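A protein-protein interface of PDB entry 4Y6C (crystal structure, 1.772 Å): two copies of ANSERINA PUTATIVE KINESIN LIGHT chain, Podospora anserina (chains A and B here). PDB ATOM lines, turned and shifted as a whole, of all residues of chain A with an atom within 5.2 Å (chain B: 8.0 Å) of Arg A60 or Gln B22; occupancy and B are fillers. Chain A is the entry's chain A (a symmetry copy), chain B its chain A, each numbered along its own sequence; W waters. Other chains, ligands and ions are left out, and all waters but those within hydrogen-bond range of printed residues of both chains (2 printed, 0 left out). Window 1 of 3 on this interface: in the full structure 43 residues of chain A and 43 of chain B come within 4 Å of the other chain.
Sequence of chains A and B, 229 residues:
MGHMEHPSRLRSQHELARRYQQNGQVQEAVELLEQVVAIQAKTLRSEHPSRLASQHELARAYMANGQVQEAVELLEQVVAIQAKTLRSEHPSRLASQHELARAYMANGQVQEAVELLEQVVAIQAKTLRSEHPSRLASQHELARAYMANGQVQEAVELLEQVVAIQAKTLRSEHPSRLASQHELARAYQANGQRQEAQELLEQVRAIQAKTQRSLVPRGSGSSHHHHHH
Water W1 bridges O of Gln B22 (3.0 Å) and NH1 of Arg A102 (3.4 Å). Water W2 lies within hydrogen-bond range of the guanidinium group of Arg A60 (3.1 Å) and the side-chain amide oxygen of Gln B22 (3.5 Å).
Of the printed residues of chain B, Arg A102 touches Gln B22 (2.8 Å) and Asn B23 (3.9 Å). Of the printed residues of chain B, Glu A99 touches Gln B22 (3.5 Å). Printed residues of chain A within 4 Å of Asn B23: Arg A102. Gly B24 touches none of the printed residues of chain A. The nearest printed residue of chain A that does not touch Gln B22 is Met A63 (6.2 Å). The nearest printed residue of chain B that does not touch Arg A102 is Arg B19 (5.8 Å).
The side-chain amide nitrogen (NE2) of Gln B22 sits close to the guanidinium group (NH2) of Arg A60 (3.1 Å). OE2 of Glu A99 lies within hydrogen-bond range of NE2 of Gln B22, 3.5 Å away. The guanidinium group (NH1) of Arg A102 sits at hydrogen-bond distance from the backbone carbonyl oxygen (O) of Gln B22.
Of the 14 printed residues of chain B, 2 touch a printed residue of chain A. Printed residues of chain A that touch a printed residue of chain B: Arg A60, Glu A99 and Arg A102. Among the printed residues, 4 pairs touch across the chains. Among the printed residues, no Asp or Glu carboxylate lies within 4 Å of a Lys or Arg side-chain nitrogen of the other chain.
Among the printed residues, pairs that only touch across the chains: Arg A102 with Asn B23.
The side-chain amide nitrogen (ND2) of Asn B23 lies within hydrogen-bond range of the backbone carbonyl oxygen (O) of Arg B19, at 2.8 Å. O of Asn B23 lies close to OE1 of Gln B25, at 3.4 Å. The side-chain carboxylate of Glu A57 lies within salt-bridge range of the guanidinium group of Arg A60 (3.7 Å). The side-chain carboxylate (OE1) of Glu A99 is in salt-bridge range of the guanidinium group (NE) of Arg A60, at 3.8 Å. The guanidinium group (NH2) of Arg A102 lies close to the side-chain sulfur (SD) of Met A63 (3.4 Å). The side-chain carboxylate (OE2) of Glu A99 lies within salt-bridge range of the guanidinium group (NE) of Arg A102.
2 positions are printed for both chains.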
ATOM      1  N   GLN A  21       2.231  17.244  35.750  1.00  0.00           N
ATOM      2  CA  GLN A  21       2.084  17.427  34.306  1.00  0.00           C
ATOM      3  C   GLN A  21       1.725  18.860  33.948  1.00  0.00           C
ATOM      4  O   GLN A  21       2.304  19.440  33.032  1.00  0.00           O
ATOM      5  CB  GLN A  21       1.021  16.474  33.754  1.00  0.00           C
ATOM      6  CG  GLN A  21       1.485  15.037  33.799  1.00  0.00           C
ATOM      7  CD  GLN A  21       0.366  14.028  33.780  1.00  0.00           C
ATOM      8  OE1 GLN A  21      -0.814  14.374  33.883  1.00  0.00           O
ATOM      9  NE2 GLN A  21       0.736  12.748  33.642  1.00  0.00           N
ATOM     10  N   GLN A  55      -2.672   1.602  35.822  1.00  0.00           N
ATOM     11  CA  GLN A  55      -1.988   1.330  34.549  1.00  0.00           C
ATOM     12  C   GLN A  55      -2.479   2.295  33.469  1.00  0.00           C
ATOM     13  O   GLN A  55      -1.698   2.815  32.685  1.00  0.00           O
ATOM     14  CB  GLN A  55      -2.210  -0.118  34.105  1.00  0.00           C
ATOM     15  CG  GLN A  55      -1.451  -1.122  34.955  1.00  0.00           C
ATOM     16  CD  GLN A  55      -1.876  -2.545  34.651  1.00  0.00           C
ATOM     17  OE1 GLN A  55      -3.040  -2.894  34.808  1.00  0.00           O
ATOM     18  NE2 GLN A  55      -0.937  -3.365  34.198  1.00  0.00           N
ATOM     19  N   HIS A  56      -3.783   2.542  33.451  1.00  0.00           N
ATOM     20  CA  HIS A  56      -4.378   3.520  32.538  1.00  0.00           C
ATOM     21  C   HIS A  56      -3.770   4.919  32.743  1.00  0.00           C
ATOM     22  O   HIS A  56      -3.402   5.601  31.781  1.00  0.00           O
ATOM     23  CB  HIS A  56      -5.889   3.519  32.765  1.00  0.00           C
ATOM     24  CG  HIS A  56      -6.647   4.530  31.963  1.00  0.00           C
ATOM     25  ND1 HIS A  56      -7.361   4.192  30.834  1.00  0.00           N
ATOM     26  CD2 HIS A  56      -6.845   5.856  32.154  1.00  0.00           C
ATOM     27  CE1 HIS A  56      -7.955   5.271  30.355  1.00  0.00           C
ATOM     28  NE2 HIS A  56      -7.650   6.295  31.129  1.00  0.00           N
ATOM     29  N   GLU A  57      -3.635   5.335  33.996  1.00  0.00           N
ATOM     30  CA  GLU A  57      -3.078   6.661  34.283  1.00  0.00           C
ATOM     31  C   GLU A  57      -1.594   6.740  33.945  1.00  0.00           C
ATOM     32  O   GLU A  57      -1.105   7.781  33.484  1.00  0.00           O
ATOM     33  CB  GLU A  57      -3.292   7.026  35.750  1.00  0.00           C
ATOM     34  CG  GLU A  57      -4.749   7.259  36.112  1.00  0.00           C
ATOM     35  CD  GLU A  57      -5.372   8.387  35.312  1.00  0.00           C
ATOM     36  OE1 GLU A  57      -4.824   9.516  35.339  1.00  0.00           O
ATOM     37  OE2 GLU A  57      -6.411   8.143  34.662  1.00  0.00           O
ATOM     38  N   LEU A  58      -0.863   5.655  34.184  1.00  0.00           N
ATOM     39  CA  LEU A  58       0.541   5.637  33.794  1.00  0.00           C
ATOM     40  C   LEU A  58       0.674   5.779  32.283  1.00  0.00           C
ATOM     41  O   LEU A  58       1.555   6.501  31.785  1.00  0.00           O
ATOM     42  CB  LEU A  58       1.233   4.352  34.267  1.00  0.00           C
ATOM     43  CG  LEU A  58       2.682   4.164  33.800  1.00  0.00           C
ATOM     44  CD1 LEU A  58       3.557   5.370  34.158  1.00  0.00           C
ATOM     45  CD2 LEU A  58       3.266   2.874  34.427  1.00  0.00           C
ATOM     46  N   ALA A  59      -0.191   5.094  31.540  1.00  0.00           N
ATOM     47  CA  ALA A  59      -0.113   5.193  30.086  1.00  0.00           C
ATOM     48  C   ALA A  59      -0.395   6.622  29.652  1.00  0.00           C
ATOM     49  O   ALA A  59       0.242   7.140  28.742  1.00  0.00           O
ATOM     50  CB  ALA A  59      -1.089   4.227  29.420  1.00  0.00           C
ATOM     51  N   ARG A  60      -1.350   7.269  30.313  1.00  0.00           N
ATOM     52  CA  ARG A  60      -1.626   8.673  30.001  1.00  0.00           C
ATOM     53  C   ARG A  60      -0.406   9.535  30.316  1.00  0.00           C
ATOM     54  O   ARG A  60      -0.104  10.481  29.585  1.00  0.00           O
ATOM     55  CB  ARG A  60      -2.847   9.183  30.774  1.00  0.00           C
ATOM     56  CG  ARG A  60      -4.152   8.569  30.315  1.00  0.00           C
ATOM     57  CD  ARG A  60      -5.328   9.143  31.091  1.00  0.00           C
ATOM     58  NE  ARG A  60      -5.505  10.565  30.816  1.00  0.00           N
ATOM     59  CZ  ARG A  60      -6.455  11.318  31.355  1.00  0.00           C
ATOM     60  NH1 ARG A  60      -7.320  10.789  32.211  1.00  0.00           N
ATOM     61  NH2 ARG A  60      -6.534  12.604  31.040  1.00  0.00           N
ATOM     62  N   ALA A  61       0.303   9.206  31.395  1.00  0.00           N
ATOM     63  CA  ALA A  61       1.518   9.934  31.754  1.00  0.00           C
ATOM     64  C   ALA A  61       2.613   9.706  30.712  1.00  0.00           C
ATOM     65  O   ALA A  61       3.358  10.631  30.371  1.00  0.00           O
ATOM     66  CB  ALA A  61       2.019   9.522  33.145  1.00  0.00           C
ATOM     67  N   TYR A  62       2.735   8.470  30.238  1.00  0.00           N
ATOM     68  CA  TYR A  62       3.690   8.179  29.169  1.00  0.00           C
ATOM     69  C   TYR A  62       3.390   9.047  27.957  1.00  0.00           C
ATOM     70  O   TYR A  62       4.307   9.594  27.335  1.00  0.00           O
ATOM     71  CB  TYR A  62       3.637   6.705  28.761  1.00  0.00           C
ATOM     72  CG  TYR A  62       4.392   5.742  29.664  1.00  0.00           C
ATOM     73  CD1 TYR A  62       5.630   6.071  30.196  1.00  0.00           C
ATOM     74  CD2 TYR A  62       3.869   4.485  29.941  1.00  0.00           C
ATOM     75  CE1 TYR A  62       6.329   5.168  31.007  1.00  0.00           C
ATOM     76  CE2 TYR A  62       4.551   3.578  30.746  1.00  0.00           C
ATOM     77  CZ  TYR A  62       5.773   3.927  31.276  1.00  0.00           C
ATOM     78  OH  TYR A  62       6.441   3.015  32.067  1.00  0.00           O
ATOM     79  N   MET A  63       2.112   9.168  27.597  1.00  0.00           N
ATOM     80  CA  MET A  63       1.760   9.978  26.431  1.00  0.00           C
ATOM     81  C   MET A  63       2.177  11.429  26.635  1.00  0.00           C
ATOM     82  O   MET A  63       2.715  12.054  25.720  1.00  0.00           O
ATOM     83  CB  MET A  63       0.263   9.909  26.129  1.00  0.00           C
ATOM     84  CG  MET A  63      -0.218   8.541  25.707  1.00  0.00           C
ATOM     85  SD  MET A  63      -1.820   8.620  24.600  1.00  0.00           S
ATOM     86  CE  MET A  63      -3.016   7.570  25.718  1.00  0.00           C
ATOM     87  N   ALA A  64       1.944  11.956  27.832  1.00  0.00           N
ATOM     88  CA  ALA A  64       2.283  13.346  28.127  1.00  0.00           C
ATOM     89  C   ALA A  64       3.794  13.573  28.060  1.00  0.00           C
ATOM     90  O   ALA A  64       4.260  14.678  27.761  1.00  0.00           O
ATOM     91  CB  ALA A  64       1.729  13.743  29.497  1.00  0.00           C
ATOM     92  N   GLU A  99      -8.697   5.718  24.979  1.00  0.00           N
ATOM     93  CA  GLU A  99      -7.326   6.104  25.332  1.00  0.00           C
ATOM     94  C   GLU A  99      -6.318   5.340  24.480  1.00  0.00           C
ATOM     95  O   GLU A  99      -5.334   5.908  23.983  1.00  0.00           O
ATOM     96  CB  GLU A  99      -7.058   5.850  26.822  1.00  0.00           C
ATOM     97  CG  GLU A  99      -5.978   6.738  27.421  1.00  0.00           C
ATOM     98  CD  GLU A  99      -6.370   8.215  27.410  1.00  0.00           C
ATOM     99  OE1 GLU A  99      -7.328   8.596  28.119  1.00  0.00           O
ATOM    100  OE2 GLU A  99      -5.728   8.994  26.684  1.00  0.00           O
ATOM    101  N   ARG A 102      -6.277   6.760  21.080  1.00  0.00           N
ATOM    102  CA  ARG A 102      -5.488   7.988  21.039  1.00  0.00           C
ATOM    103  C   ARG A 102      -3.998   7.687  20.953  1.00  0.00           C
ATOM    104  O   ARG A 102      -3.268   8.353  20.205  1.00  0.00           O
ATOM    105  CB  ARG A 102      -5.766   8.865  22.261  1.00  0.00           C
ATOM    106  CG  ARG A 102      -4.894  10.121  22.304  1.00  0.00           C
ATOM    107  CD  ARG A 102      -5.306  11.084  23.407  1.00  0.00           C
ATOM    108  NE  ARG A 102      -4.913  10.651  24.748  1.00  0.00           N
ATOM    109  CZ  ARG A 102      -3.863  11.124  25.415  1.00  0.00           C
ATOM    110  NH1 ARG A 102      -3.084  12.046  24.868  1.00  0.00           N
ATOM    111  NH2 ARG A 102      -3.590  10.675  26.633  1.00  0.00           N
ATOM    112  N   GLU B  15     -15.346  18.626  30.185  1.00  0.00           N
ATOM    113  CA  GLU B  15     -14.855  17.303  29.809  1.00  0.00           C
ATOM    114  C   GLU B  15     -14.528  17.251  28.318  1.00  0.00           C
ATOM    115  O   GLU B  15     -13.538  16.630  27.912  1.00  0.00           O
ATOM    116  CB  GLU B  15     -15.881  16.210  30.164  1.00  0.00           C
ATOM    117  CG  GLU B  15     -15.494  14.814  29.660  1.00  0.00           C
ATOM    118  CD  GLU B  15     -16.402  13.694  30.183  1.00  0.00           C
ATOM    119  OE1 GLU B  15     -17.318  13.975  30.992  1.00  0.00           O
ATOM    120  OE2 GLU B  15     -16.202  12.520  29.777  1.00  0.00           O
ATOM    121  N   LEU B  16     -15.354  17.895  27.496  1.00  0.00           N
ATOM    122  CA  LEU B  16     -15.106  17.891  26.058  1.00  0.00           C
ATOM    123  C   LEU B  16     -13.810  18.651  25.773  1.00  0.00           C
ATOM    124  O   LEU B  16     -13.018  18.229  24.924  1.00  0.00           O
ATOM    125  CB  LEU B  16     -16.288  18.503  25.287  1.00  0.00           C
ATOM    126  CG  LEU B  16     -16.202  18.577  23.763  1.00  0.00           C
ATOM    127  CD1 LEU B  16     -15.966  17.204  23.116  1.00  0.00           C
ATOM    128  CD2 LEU B  16     -17.470  19.235  23.203  1.00  0.00           C
ATOM    129  N   ALA B  17     -13.583  19.754  26.494  1.00  0.00           N
ATOM    130  CA  ALA B  17     -12.350  20.531  26.316  1.00  0.00           C
ATOM    131  C   ALA B  17     -11.130  19.686  26.645  1.00  0.00           C
ATOM    132  O   ALA B  17     -10.111  19.740  25.950  1.00  0.00           O
ATOM    133  CB  ALA B  17     -12.363  21.787  27.197  1.00  0.00           C
ATOM    134  N   ARG B  18     -11.226  18.912  27.716  1.00  0.00           N
ATOM    135  CA  ARG B  18     -10.111  18.046  28.107  1.00  0.00           C
ATOM    136  C   ARG B  18      -9.819  16.973  27.063  1.00  0.00           C
ATOM    137  O   ARG B  18      -8.661  16.638  26.825  1.00  0.00           O
ATOM    138  CB  ARG B  18     -10.382  17.393  29.467  1.00  0.00           C
ATOM    139  CG  ARG B  18     -10.255  18.362  30.644  1.00  0.00           C
ATOM    140  CD  ARG B  18     -10.292  17.635  31.988  1.00  0.00           C
ATOM    141  NE  ARG B  18     -11.627  17.140  32.323  1.00  0.00           N
ATOM    142  CZ  ARG B  18     -12.550  17.859  32.958  1.00  0.00           C
ATOM    143  NH1 ARG B  18     -12.287  19.107  33.328  1.00  0.00           N
ATOM    144  NH2 ARG B  18     -13.738  17.338  33.220  1.00  0.00           N
ATOM    145  N   ARG B  19     -10.858  16.432  26.437  1.00  0.00           N
ATOM    146  CA  ARG B  19     -10.640  15.448  25.381  1.00  0.00           C
ATOM    147  C   ARG B  19      -9.941  16.098  24.190  1.00  0.00           C
ATOM    148  O   ARG B  19      -9.050  15.501  23.575  1.00  0.00           O
ATOM    149  CB  ARG B  19     -11.963  14.807  24.943  1.00  0.00           C
ATOM    150  CG  ARG B  19     -12.563  13.852  25.975  1.00  0.00           C
ATOM    151  CD  ARG B  19     -11.865  12.470  25.981  1.00  0.00           C
ATOM    152  NE  ARG B  19     -12.196  11.662  24.804  1.00  0.00           N
ATOM    153  CZ  ARG B  19     -13.290  10.916  24.703  1.00  0.00           C
ATOM    154  NH1 ARG B  19     -14.161  10.885  25.711  1.00  0.00           N
ATOM    155  NH2 ARG B  19     -13.512  10.198  23.607  1.00  0.00           N
ATOM    156  N   TYR B  20     -10.353  17.319  23.852  1.00  0.00           N
ATOM    157  CA  TYR B  20      -9.694  18.036  22.761  1.00  0.00           C
ATOM    158  C   TYR B  20      -8.214  18.225  23.070  1.00  0.00           C
ATOM    159  O   TYR B  20      -7.356  17.992  22.218  1.00  0.00           O
ATOM    160  CB  TYR B  20     -10.340  19.405  22.529  1.00  0.00           C
ATOM    161  CG  TYR B  20     -11.496  19.411  21.551  1.00  0.00           C
ATOM    162  CD1 TYR B  20     -11.419  18.721  20.350  1.00  0.00           C
ATOM    163  CD2 TYR B  20     -12.649  20.141  21.817  1.00  0.00           C
ATOM    164  CE1 TYR B  20     -12.473  18.742  19.448  1.00  0.00           C
ATOM    165  CE2 TYR B  20     -13.702  20.169  20.928  1.00  0.00           C
ATOM    166  CZ  TYR B  20     -13.613  19.464  19.747  1.00  0.00           C
ATOM    167  OH  TYR B  20     -14.666  19.490  18.863  1.00  0.00           O
ATOM    168  N   GLN B  21      -7.924  18.681  24.286  1.00  0.00           N
ATOM    169  CA  GLN B  21      -6.545  18.947  24.695  1.00  0.00           C
ATOM    170  C   GLN B  21      -5.681  17.697  24.629  1.00  0.00           C
ATOM    171  O   GLN B  21      -4.563  17.735  24.119  1.00  0.00           O
ATOM    172  CB  GLN B  21      -6.511  19.525  26.111  1.00  0.00           C
ATOM    173  CG  GLN B  21      -7.080  20.923  26.155  1.00  0.00           C
ATOM    174  CD  GLN B  21      -7.561  21.350  27.518  1.00  0.00           C
ATOM    175  OE1 GLN B  21      -7.621  20.552  28.457  1.00  0.00           O
ATOM    176  NE2 GLN B  21      -7.910  22.638  27.638  1.00  0.00           N
ATOM    177  N   GLN B  22      -6.213  16.595  25.142  1.00  0.00           N
ATOM    178  CA  GLN B  22      -5.500  15.321  25.132  1.00  0.00           C
ATOM    179  C   GLN B  22      -5.167  14.887  23.712  1.00  0.00           C
ATOM    180  O   GLN B  22      -4.167  14.207  23.488  1.00  0.00           O
ATOM    181  CB  GLN B  22      -6.325  14.231  25.808  1.00  0.00           C
ATOM    182  CG  GLN B  22      -6.526  14.402  27.296  1.00  0.00           C
ATOM    183  CD  GLN B  22      -7.286  13.241  27.892  1.00  0.00           C
ATOM    184  OE1 GLN B  22      -8.452  13.372  28.265  1.00  0.00           O
ATOM    185  NE2 GLN B  22      -6.630  12.089  27.980  1.00  0.00           N
ATOM    186  N   ASN B  23      -6.013  15.268  22.760  1.00  0.00           N
ATOM    187  CA  ASN B  23      -5.813  14.891  21.362  1.00  0.00           C
ATOM    188  C   ASN B  23      -4.959  15.889  20.603  1.00  0.00           C
ATOM    189  O   ASN B  23      -4.779  15.765  19.387  1.00  0.00           O
ATOM    190  CB  ASN B  23      -7.154  14.739  20.653  1.00  0.00           C
ATOM    191  CG  ASN B  23      -7.779  13.392  20.899  1.00  0.00           C
ATOM    192  OD1 ASN B  23      -7.384  12.391  20.290  1.00  0.00           O
ATOM    193  ND2 ASN B  23      -8.749  13.349  21.800  1.00  0.00           N
ATOM    194  N   GLY B  24      -4.463  16.890  21.321  1.00  0.00           N
ATOM    195  CA  GLY B  24      -3.608  17.904  20.733  1.00  0.00           C
ATOM    196  C   GLY B  24      -4.355  19.119  20.206  1.00  0.00           C
ATOM    197  O   GLY B  24      -3.729  20.091  19.790  1.00  0.00           O
ATOM    198  N   GLN B  25      -5.687  19.058  20.205  1.00  0.00           N
ATOM    199  CA  GLN B  25      -6.520  20.151  19.700  1.00  0.00           C
ATOM    200  C   GLN B  25      -6.700  21.230  20.765  1.00  0.00           C
ATOM    201  O   GLN B  25      -7.819  21.559  21.154  1.00  0.00           O
ATOM    202  CB  GLN B  25      -7.891  19.636  19.247  1.00  0.00           C
ATOM    203  CG  GLN B  25      -7.947  19.148  17.800  1.00  0.00           C
ATOM    204  CD  GLN B  25      -7.144  17.891  17.566  1.00  0.00           C
ATOM    205  OE1 GLN B  25      -7.599  16.783  17.862  1.00  0.00           O
ATOM    206  NE2 GLN B  25      -5.941  18.051  17.024  1.00  0.00           N
ATOM    207  N   VAL B  26      -5.593  21.783  21.241  1.00  0.00           N
ATOM    208  CA  VAL B  26      -5.668  22.765  22.321  1.00  0.00           C
ATOM    209  C   VAL B  26      -6.359  24.066  21.878  1.00  0.00           C
ATOM    210  O   VAL B  26      -7.004  24.732  22.686  1.00  0.00           O
ATOM    211  CB  VAL B  26      -4.261  23.068  22.893  1.00  0.00           C
ATOM    212  CG1 VAL B  26      -3.754  21.875  23.698  1.00  0.00           C
ATOM    213  CG2 VAL B  26      -3.274  23.414  21.778  1.00  0.00           C
ATOM    214  N   ALA B  29     -10.159  23.570  22.090  1.00  0.00           N
ATOM    215  CA  ALA B  29     -10.608  23.614  23.484  1.00  0.00           C
ATOM    216  C   ALA B  29     -10.792  25.063  23.948  1.00  0.00           C
ATOM    217  O   ALA B  29     -11.736  25.387  24.676  1.00  0.00           O
ATOM    218  CB  ALA B  29      -9.616  22.901  24.391  1.00  0.00           C
ATOM    219  N   ALA B  64      -2.807  25.728  28.147  1.00  0.00           N
ATOM    220  CA  ALA B  64      -2.496  24.575  27.305  1.00  0.00           C
ATOM    221  C   ALA B  64      -2.212  25.001  25.864  1.00  0.00           C
ATOM    222  O   ALA B  64      -1.461  24.339  25.140  1.00  0.00           O
ATOM    223  CB  ALA B  64      -3.640  23.559  27.362  1.00  0.00           C
HETATM  224  O   HOH W   1      -2.453  12.667  21.616  1.00  0.00           O
HETATM  225  O   HOH W   2      -6.742  15.586  30.366  1.00  0.00           O
